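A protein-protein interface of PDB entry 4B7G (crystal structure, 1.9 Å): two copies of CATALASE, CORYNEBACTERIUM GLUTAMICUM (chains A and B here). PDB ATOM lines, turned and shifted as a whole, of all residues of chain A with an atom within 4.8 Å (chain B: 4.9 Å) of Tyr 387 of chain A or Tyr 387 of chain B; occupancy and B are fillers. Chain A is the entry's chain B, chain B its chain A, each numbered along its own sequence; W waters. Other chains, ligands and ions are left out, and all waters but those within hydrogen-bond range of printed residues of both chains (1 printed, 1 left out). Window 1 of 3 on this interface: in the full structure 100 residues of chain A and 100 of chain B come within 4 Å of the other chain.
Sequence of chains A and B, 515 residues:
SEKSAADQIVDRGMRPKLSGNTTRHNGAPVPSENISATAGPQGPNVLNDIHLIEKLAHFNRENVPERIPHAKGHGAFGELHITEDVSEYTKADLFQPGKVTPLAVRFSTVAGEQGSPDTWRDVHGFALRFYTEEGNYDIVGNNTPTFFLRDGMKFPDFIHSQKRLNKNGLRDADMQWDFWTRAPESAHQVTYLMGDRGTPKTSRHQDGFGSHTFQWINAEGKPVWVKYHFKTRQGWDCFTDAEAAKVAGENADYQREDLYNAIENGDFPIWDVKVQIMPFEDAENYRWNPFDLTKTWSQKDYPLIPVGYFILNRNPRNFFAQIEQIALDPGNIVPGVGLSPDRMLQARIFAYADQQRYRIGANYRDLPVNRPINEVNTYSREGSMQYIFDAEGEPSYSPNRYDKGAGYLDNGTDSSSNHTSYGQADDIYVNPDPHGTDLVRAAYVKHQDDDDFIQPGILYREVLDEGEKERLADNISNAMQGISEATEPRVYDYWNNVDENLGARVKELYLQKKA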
ATOM      1  N   GLY A  13      -3.707 -21.923 -27.244  1.00  0.00           N
ATOM      2  CA  GLY A  13      -2.765 -22.981 -26.913  1.00  0.00           C
ATOM      3  C   GLY A  13      -1.315 -22.742 -27.311  1.00  0.00           C
ATOM      4  O   GLY A  13      -0.427 -23.531 -26.956  1.00  0.00           O
ATOM      5  N   ASP A 366     -12.097 -30.904 -26.134  1.00  0.00           N
ATOM      6  CA  ASP A 366     -11.498 -29.860 -25.309  1.00  0.00           C
ATOM      7  C   ASP A 366     -10.255 -29.234 -25.928  1.00  0.00           C
ATOM      8  O   ASP A 366      -9.756 -28.228 -25.425  1.00  0.00           O
ATOM      9  CB  ASP A 366     -11.149 -30.403 -23.922  1.00  0.00           C
ATOM     10  CG  ASP A 366     -12.374 -30.810 -23.124  1.00  0.00           C
ATOM     11  OD1 ASP A 366     -13.464 -30.242 -23.354  1.00  0.00           O
ATOM     12  OD2 ASP A 366     -12.239 -31.688 -22.240  1.00  0.00           O
ATOM     13  N   LEU A 367      -9.737 -29.827 -27.003  1.00  0.00           N
ATOM     14  CA  LEU A 367      -8.557 -29.263 -27.652  1.00  0.00           C
ATOM     15  C   LEU A 367      -8.910 -27.913 -28.275  1.00  0.00           C
ATOM     16  O   LEU A 367     -10.039 -27.719 -28.738  1.00  0.00           O
ATOM     17  CB  LEU A 367      -8.004 -30.213 -28.720  1.00  0.00           C
ATOM     18  CG  LEU A 367      -7.480 -31.568 -28.232  1.00  0.00           C
ATOM     19  CD1 LEU A 367      -7.142 -32.449 -29.425  1.00  0.00           C
ATOM     20  CD2 LEU A 367      -6.238 -31.375 -27.349  1.00  0.00           C
ATOM     21  N   PRO A 368      -7.946 -26.979 -28.287  1.00  0.00           N
ATOM     22  CA  PRO A 368      -8.171 -25.602 -28.751  1.00  0.00           C
ATOM     23  C   PRO A 368      -8.965 -25.502 -30.056  1.00  0.00           C
ATOM     24  O   PRO A 368      -9.937 -24.739 -30.118  1.00  0.00           O
ATOM     25  CB  PRO A 368      -6.745 -25.085 -28.950  1.00  0.00           C
ATOM     26  CG  PRO A 368      -5.978 -25.748 -27.833  1.00  0.00           C
ATOM     27  CD  PRO A 368      -6.584 -27.152 -27.739  1.00  0.00           C
ATOM     28  N   ARG A 371     -12.820 -26.627 -29.513  1.00  0.00           N
ATOM     29  CA  ARG A 371     -13.742 -25.928 -28.603  1.00  0.00           C
ATOM     30  C   ARG A 371     -14.540 -24.858 -29.342  1.00  0.00           C
ATOM     31  O   ARG A 371     -13.987 -24.143 -30.171  1.00  0.00           O
ATOM     32  CB  ARG A 371     -12.981 -25.250 -27.464  1.00  0.00           C
ATOM     33  CG  ARG A 371     -12.330 -26.194 -26.483  1.00  0.00           C
ATOM     34  CD  ARG A 371     -12.023 -25.451 -25.178  1.00  0.00           C
ATOM     35  NE  ARG A 371     -11.132 -24.311 -25.383  1.00  0.00           N
ATOM     36  CZ  ARG A 371      -9.803 -24.393 -25.335  1.00  0.00           C
ATOM     37  NH1 ARG A 371      -9.222 -25.562 -25.086  1.00  0.00           N
ATOM     38  NH2 ARG A 371      -9.052 -23.314 -25.523  1.00  0.00           N
ATOM     39  N   MET A 385      -6.702 -37.471 -20.001  1.00  0.00           N
ATOM     40  CA  MET A 385      -6.204 -36.137 -20.340  1.00  0.00           C
ATOM     41  C   MET A 385      -7.279 -35.066 -20.206  1.00  0.00           C
ATOM     42  O   MET A 385      -7.526 -34.305 -21.157  1.00  0.00           O
ATOM     43  CB  MET A 385      -5.675 -36.128 -21.785  1.00  0.00           C
ATOM     44  CG  MET A 385      -4.376 -36.906 -21.976  1.00  0.00           C
ATOM     45  SD  MET A 385      -2.982 -36.074 -21.161  1.00  0.00           S
ATOM     46  CE  MET A 385      -2.764 -34.706 -22.275  1.00  0.00           C
ATOM     47  N   GLN A 386      -7.936 -35.008 -19.052  1.00  0.00           N
ATOM     48  CA  GLN A 386      -8.926 -33.955 -18.831  1.00  0.00           C
ATOM     49  C   GLN A 386      -8.223 -32.654 -18.468  1.00  0.00           C
ATOM     50  O   GLN A 386      -7.712 -32.500 -17.349  1.00  0.00           O
ATOM     51  CB  GLN A 386      -9.920 -34.327 -17.727  1.00  0.00           C
ATOM     52  CG  GLN A 386     -10.891 -33.182 -17.424  1.00  0.00           C
ATOM     53  CD  GLN A 386     -11.879 -33.491 -16.314  1.00  0.00           C
ATOM     54  OE1 GLN A 386     -11.662 -34.395 -15.507  1.00  0.00           O
ATOM     55  NE2 GLN A 386     -12.972 -32.726 -16.262  1.00  0.00           N
ATOM     56  N   TYR A 387      -8.182 -31.727 -19.422  1.00  0.00           N
ATOM     57  CA  TYR A 387      -7.549 -30.432 -19.180  1.00  0.00           C
ATOM     58  C   TYR A 387      -8.530 -29.468 -18.548  1.00  0.00           C
ATOM     59  O   TYR A 387      -8.164 -28.710 -17.639  1.00  0.00           O
ATOM     60  CB  TYR A 387      -7.038 -29.830 -20.485  1.00  0.00           C
ATOM     61  CG  TYR A 387      -6.157 -28.606 -20.338  1.00  0.00           C
ATOM     62  CD1 TYR A 387      -6.677 -27.385 -19.904  1.00  0.00           C
ATOM     63  CD2 TYR A 387      -4.812 -28.656 -20.675  1.00  0.00           C
ATOM     64  CE1 TYR A 387      -5.878 -26.276 -19.781  1.00  0.00           C
ATOM     65  CE2 TYR A 387      -4.012 -27.543 -20.566  1.00  0.00           C
ATOM     66  CZ  TYR A 387      -4.551 -26.359 -20.125  1.00  0.00           C
ATOM     67  OH  TYR A 387      -3.751 -25.245 -20.006  1.00  0.00           O
ATOM     68  N   ILE A 388      -9.776 -29.502 -19.009  1.00  0.00           N
ATOM     69  CA  ILE A 388     -10.797 -28.555 -18.570  1.00  0.00           C
ATOM     70  C   ILE A 388     -11.831 -29.222 -17.662  1.00  0.00           C
ATOM     71  O   ILE A 388     -12.332 -30.316 -17.964  1.00  0.00           O
ATOM     72  CB  ILE A 388     -11.518 -27.945 -19.799  1.00  0.00           C
ATOM     73  CG1 ILE A 388     -10.517 -27.178 -20.662  1.00  0.00           C
ATOM     74  CG2 ILE A 388     -12.672 -27.034 -19.369  1.00  0.00           C
ATOM     75  CD1 ILE A 388     -11.112 -26.672 -21.980  1.00  0.00           C
ATOM     76  N   PHE A 389     -12.148 -28.567 -16.549  1.00  0.00           N
ATOM     77  CA  PHE A 389     -13.153 -29.093 -15.634  1.00  0.00           C
ATOM     78  C   PHE A 389     -14.115 -28.005 -15.160  1.00  0.00           C
ATOM     79  O   PHE A 389     -13.808 -26.807 -15.229  1.00  0.00           O
ATOM     80  CB  PHE A 389     -12.495 -29.785 -14.438  1.00  0.00           C
ATOM     81  CG  PHE A 389     -11.471 -28.941 -13.720  1.00  0.00           C
ATOM     82  CD1 PHE A 389     -10.139 -28.944 -14.125  1.00  0.00           C
ATOM     83  CD2 PHE A 389     -11.834 -28.173 -12.622  1.00  0.00           C
ATOM     84  CE1 PHE A 389      -9.185 -28.174 -13.450  1.00  0.00           C
ATOM     85  CE2 PHE A 389     -10.900 -27.406 -11.945  1.00  0.00           C
ATOM     86  CZ  PHE A 389      -9.576 -27.408 -12.351  1.00  0.00           C
ATOM     87  N   GLY B  13      -7.418 -24.212 -15.664  1.00  0.00           N
ATOM     88  CA  GLY B  13      -8.292 -25.168 -16.321  1.00  0.00           C
ATOM     89  C   GLY B  13      -9.742 -25.195 -15.857  1.00  0.00           C
ATOM     90  O   GLY B  13     -10.564 -25.897 -16.455  1.00  0.00           O
ATOM     91  N   ASP B 366       1.471 -31.607 -19.912  1.00  0.00           N
ATOM     92  CA  ASP B 366       0.789 -30.368 -20.275  1.00  0.00           C
ATOM     93  C   ASP B 366      -0.462 -30.089 -19.446  1.00  0.00           C
ATOM     94  O   ASP B 366      -0.989 -28.971 -19.475  1.00  0.00           O
ATOM     95  CB  ASP B 366       0.432 -30.386 -21.761  1.00  0.00           C
ATOM     96  CG  ASP B 366       1.661 -30.399 -22.649  1.00  0.00           C
ATOM     97  OD1 ASP B 366       2.747 -29.970 -22.194  1.00  0.00           O
ATOM     98  OD2 ASP B 366       1.537 -30.831 -23.810  1.00  0.00           O
ATOM     99  N   LEU B 367      -0.940 -31.090 -18.712  1.00  0.00           N
ATOM    100  CA  LEU B 367      -2.143 -30.915 -17.894  1.00  0.00           C
ATOM    101  C   LEU B 367      -1.841 -29.877 -16.824  1.00  0.00           C
ATOM    102  O   LEU B 367      -0.721 -29.835 -16.298  1.00  0.00           O
ATOM    103  CB  LEU B 367      -2.569 -32.239 -17.248  1.00  0.00           C
ATOM    104  CG  LEU B 367      -3.057 -33.338 -18.191  1.00  0.00           C
ATOM    105  CD1 LEU B 367      -3.415 -34.589 -17.404  1.00  0.00           C
ATOM    106  CD2 LEU B 367      -4.269 -32.848 -18.989  1.00  0.00           C
ATOM    107  N   PRO B 368      -2.826 -29.019 -16.515  1.00  0.00           N
ATOM    108  CA  PRO B 368      -2.634 -27.905 -15.574  1.00  0.00           C
ATOM    109  C   PRO B 368      -1.813 -28.244 -14.318  1.00  0.00           C
ATOM    110  O   PRO B 368      -0.871 -27.516 -13.994  1.00  0.00           O
ATOM    111  CB  PRO B 368      -4.070 -27.537 -15.193  1.00  0.00           C
ATOM    112  CG  PRO B 368      -4.865 -27.822 -16.468  1.00  0.00           C
ATOM    113  CD  PRO B 368      -4.185 -29.027 -17.105  1.00  0.00           C
ATOM    114  N   ARG B 371       2.032 -28.850 -15.176  1.00  0.00           N
ATOM    115  CA  ARG B 371       2.843 -27.776 -15.758  1.00  0.00           C
ATOM    116  C   ARG B 371       3.567 -27.001 -14.658  1.00  0.00           C
ATOM    117  O   ARG B 371       2.975 -26.689 -13.619  1.00  0.00           O
ATOM    118  CB  ARG B 371       1.970 -26.784 -16.545  1.00  0.00           C
ATOM    119  CG  ARG B 371       1.361 -27.325 -17.830  1.00  0.00           C
ATOM    120  CD  ARG B 371       1.090 -26.180 -18.818  1.00  0.00           C
ATOM    121  NE  ARG B 371       0.187 -25.167 -18.277  1.00  0.00           N
ATOM    122  CZ  ARG B 371      -1.138 -25.288 -18.231  1.00  0.00           C
ATOM    123  NH1 ARG B 371      -1.724 -26.387 -18.691  1.00  0.00           N
ATOM    124  NH2 ARG B 371      -1.888 -24.312 -17.721  1.00  0.00           N
ATOM    125  N   MET B 385      -3.490 -35.855 -28.078  1.00  0.00           N
ATOM    126  CA  MET B 385      -4.048 -34.779 -27.268  1.00  0.00           C
ATOM    127  C   MET B 385      -3.068 -33.646 -26.981  1.00  0.00           C
ATOM    128  O   MET B 385      -2.919 -33.240 -25.824  1.00  0.00           O
ATOM    129  CB  MET B 385      -4.593 -35.350 -25.948  1.00  0.00           C
ATOM    130  CG  MET B 385      -5.852 -36.204 -26.125  1.00  0.00           C
ATOM    131  SD  MET B 385      -7.318 -35.224 -26.561  1.00  0.00           S
ATOM    132  CE  MET B 385      -7.604 -34.273 -25.082  1.00  0.00           C
ATOM    133  N   GLN B 386      -2.405 -33.130 -28.018  1.00  0.00           N
ATOM    134  CA  GLN B 386      -1.519 -31.983 -27.824  1.00  0.00           C
ATOM    135  C   GLN B 386      -2.345 -30.714 -27.685  1.00  0.00           C
ATOM    136  O   GLN B 386      -2.988 -30.267 -28.644  1.00  0.00           O
ATOM    137  CB  GLN B 386      -0.530 -31.828 -28.984  1.00  0.00           C
ATOM    138  CG  GLN B 386       0.445 -30.657 -28.774  1.00  0.00           C
ATOM    139  CD  GLN B 386       1.394 -30.447 -29.953  1.00  0.00           C
ATOM    140  OE1 GLN B 386       1.163 -30.948 -31.061  1.00  0.00           O
ATOM    141  NE2 GLN B 386       2.477 -29.707 -29.712  1.00  0.00           N
ATOM    142  N   TYR B 387      -2.341 -30.150 -26.483  1.00  0.00           N
ATOM    143  CA  TYR B 387      -3.082 -28.921 -26.234  1.00  0.00           C
ATOM    144  C   TYR B 387      -2.178 -27.730 -26.447  1.00  0.00           C
ATOM    145  O   TYR B 387      -2.584 -26.744 -27.052  1.00  0.00           O
ATOM    146  CB  TYR B 387      -3.596 -28.892 -24.799  1.00  0.00           C
ATOM    147  CG  TYR B 387      -4.581 -27.788 -24.491  1.00  0.00           C
ATOM    148  CD1 TYR B 387      -4.188 -26.445 -24.463  1.00  0.00           C
ATOM    149  CD2 TYR B 387      -5.902 -28.089 -24.189  1.00  0.00           C
ATOM    150  CE1 TYR B 387      -5.090 -25.447 -24.175  1.00  0.00           C
ATOM    151  CE2 TYR B 387      -6.806 -27.096 -23.884  1.00  0.00           C
ATOM    152  CZ  TYR B 387      -6.401 -25.783 -23.879  1.00  0.00           C
ATOM    153  OH  TYR B 387      -7.315 -24.805 -23.584  1.00  0.00           O
ATOM    154  N   ILE B 388      -0.946 -27.825 -25.962  1.00  0.00           N
ATOM    155  CA  ILE B 388      -0.001 -26.718 -26.004  1.00  0.00           C
ATOM    156  C   ILE B 388       1.027 -26.949 -27.103  1.00  0.00           C
ATOM    157  O   ILE B 388       1.559 -28.050 -27.236  1.00  0.00           O
ATOM    158  CB  ILE B 388       0.706 -26.591 -24.637  1.00  0.00           C
ATOM    159  CG1 ILE B 388      -0.331 -26.426 -23.524  1.00  0.00           C
ATOM    160  CG2 ILE B 388       1.693 -25.429 -24.618  1.00  0.00           C
ATOM    161  CD1 ILE B 388       0.283 -26.472 -22.143  1.00  0.00           C
ATOM    162  N   PHE B 389       1.307 -25.919 -27.899  1.00  0.00           N
ATOM    163  CA  PHE B 389       2.289 -26.049 -28.973  1.00  0.00           C
ATOM    164  C   PHE B 389       3.152 -24.804 -29.052  1.00  0.00           C
ATOM    165  O   PHE B 389       2.762 -23.740 -28.549  1.00  0.00           O
ATOM    166  CB  PHE B 389       1.611 -26.344 -30.320  1.00  0.00           C
ATOM    167  CG  PHE B 389       0.569 -25.332 -30.719  1.00  0.00           C
ATOM    168  CD1 PHE B 389       0.919 -24.196 -31.456  1.00  0.00           C
ATOM    169  CD2 PHE B 389      -0.762 -25.521 -30.372  1.00  0.00           C
ATOM    170  CE1 PHE B 389      -0.042 -23.265 -31.832  1.00  0.00           C
ATOM    171  CE2 PHE B 389      -1.731 -24.595 -30.740  1.00  0.00           C
ATOM    172  CZ  PHE B 389      -1.368 -23.460 -31.467  1.00  0.00           C
HETATM  173  O   HOH W   1      -6.586 -22.382 -25.043  1.00  0.00           O
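O of Gly 13 of chain B is in hydrogen-bond range of N of Phe 389 of chain A (3.1 Å). N of Phe 389 of chain B sits at hydrogen-bond distance from O of Gly 13 of chain A, at 3.1 Å. The guanidinium group (NH1) of Arg 371 of chain A lies within hydrogen-bond range of the side-chain hydroxyl (OH) of Tyr 387 of chain B (2.5 Å). The guanidinium group (NH1) of Arg 371 of chain B is in hydrogen-bond range of the side-chain hydroxyl (OH) of Tyr 387 of chain A (2.7 Å).
The backbone carbonyl oxygen of Ile 388 of chain B lies within hydrogen-bond range of the side-chain amide nitrogen of Gln 386 of chain B. NE2 of Gln 386 of chain A is in hydrogen-bond range of O of Ile 388 of chain A, at 3.0 Å. The guanidinium group (NH1) of Arg 371 of chain A is in hydrogen-bond range of the backbone carbonyl oxygen (O) of Asp 366 of chain A (2.7 Å). The backbone carbonyl oxygen (O) of Asp 366 of chain B lies within hydrogen-bond range of the guanidinium group (NH1) of Arg 371 of chain B.
Among the printed residues, pairs that only touch across the chains: Gly 13 of chain A with Ile 388 of chain B, Ile 388 of chain A with Gly 13 of chain B, Asp 366 of chain A with Tyr 387 of chain B, Tyr 387 of chain A with Asp 366 of chain B, Tyr 387 of chain A with Pro 368 of chain B, Pro 368 of chain A with Tyr 387 of chain B, Leu 367 of chain A with Gln 386 of chain B, Tyr 387 of chain A with Tyr 387 of chain B, Gly 13 of chain A with Tyr 387 of chain B, Tyr 387 of chain A with Gly 13 of chain B, Gln 386 of chain A with Leu 367 of chain B, Met 385 of chain A with Met 385 of chain B, Leu 367 of chain A with Met 385 of chain B and Met 385 of chain A with Leu 367 of chain B.
Printed residues of chain B within 4 Å of Asp 366 of chain A: Tyr 387. Printed residues of chain B within 4 Å of Tyr 387 of chain A: Gly 13, Asp 366, Pro 368, Arg 371 and Tyr 387. Of the printed residues of chain B, Ile 388 of chain A touches Gly 13. Printed residues of chain A within 4 Å of Pro 368 of chain B: Tyr 387. Of the printed residues of chain A, Tyr 387 of chain B touches Gly 13, Asp 366, Pro 368, Arg 371 and Tyr 387. Of the printed residues of chain A, Phe 389 of chain B touches Gly 13 (3.1 Å). The nearest printed residue of chain B that does not touch Ile 388 of chain A is Tyr 387 of chain B (4.5 Å).
Of the 10 printed residues of chain B, 10 touch a printed residue of chain A. Printed residues of chain B that touch a printed residue of chain A: Gly 13, Asp 366, Leu 367, Pro 368, Arg 371, Met 385, Gln 386, Tyr 387, Ile 388 and Phe 389. Hydrophobic or aromatic side chains of chain B that line the printed part of chain A: Leu 367, Pro 368, Met 385, Tyr 387, Ile 388 and Phe 389. Along chain A the printed residues that touch a printed residue of chain B span positions 13 to 389. Among the printed residues, 18 pairs touch across the chains. Among the printed residues, no Asp or Glu carboxylate lies within 4 Å of a Lys or Arg side-chain nitrogen of the other chain.
Gly 13 of chain A touches Ile 388 of chain B, and with the chains exchanged Ile 388 of chain A touches Gly 13 of chain B. Pro 368 of chain A touches Tyr 387 of chain B, and with the chains exchanged Tyr 387 of chain A touches Pro 368 of chain B. Arg 371 of chain A touches Tyr 387 of chain B, and with the chains exchanged Tyr 387 of chain A touches Arg 371 of chain B. Met 385 of chain B touches its own counterpart, Met 385 of chain A. Positions printed for both chains: 13, 366, 367, 368, 371, 385, 386, 387, 388 and 389. Of the 18 pairs that touch across the chains among the printed residues, 18 have their exchanged pair printed and touching as well.
Water W1 lies within hydrogen-bond range of the guanidinium group of Arg 371 of chain A (2.7 Å) and the side-chain hydroxyl of Tyr 387 of chain B (2.9 Å).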
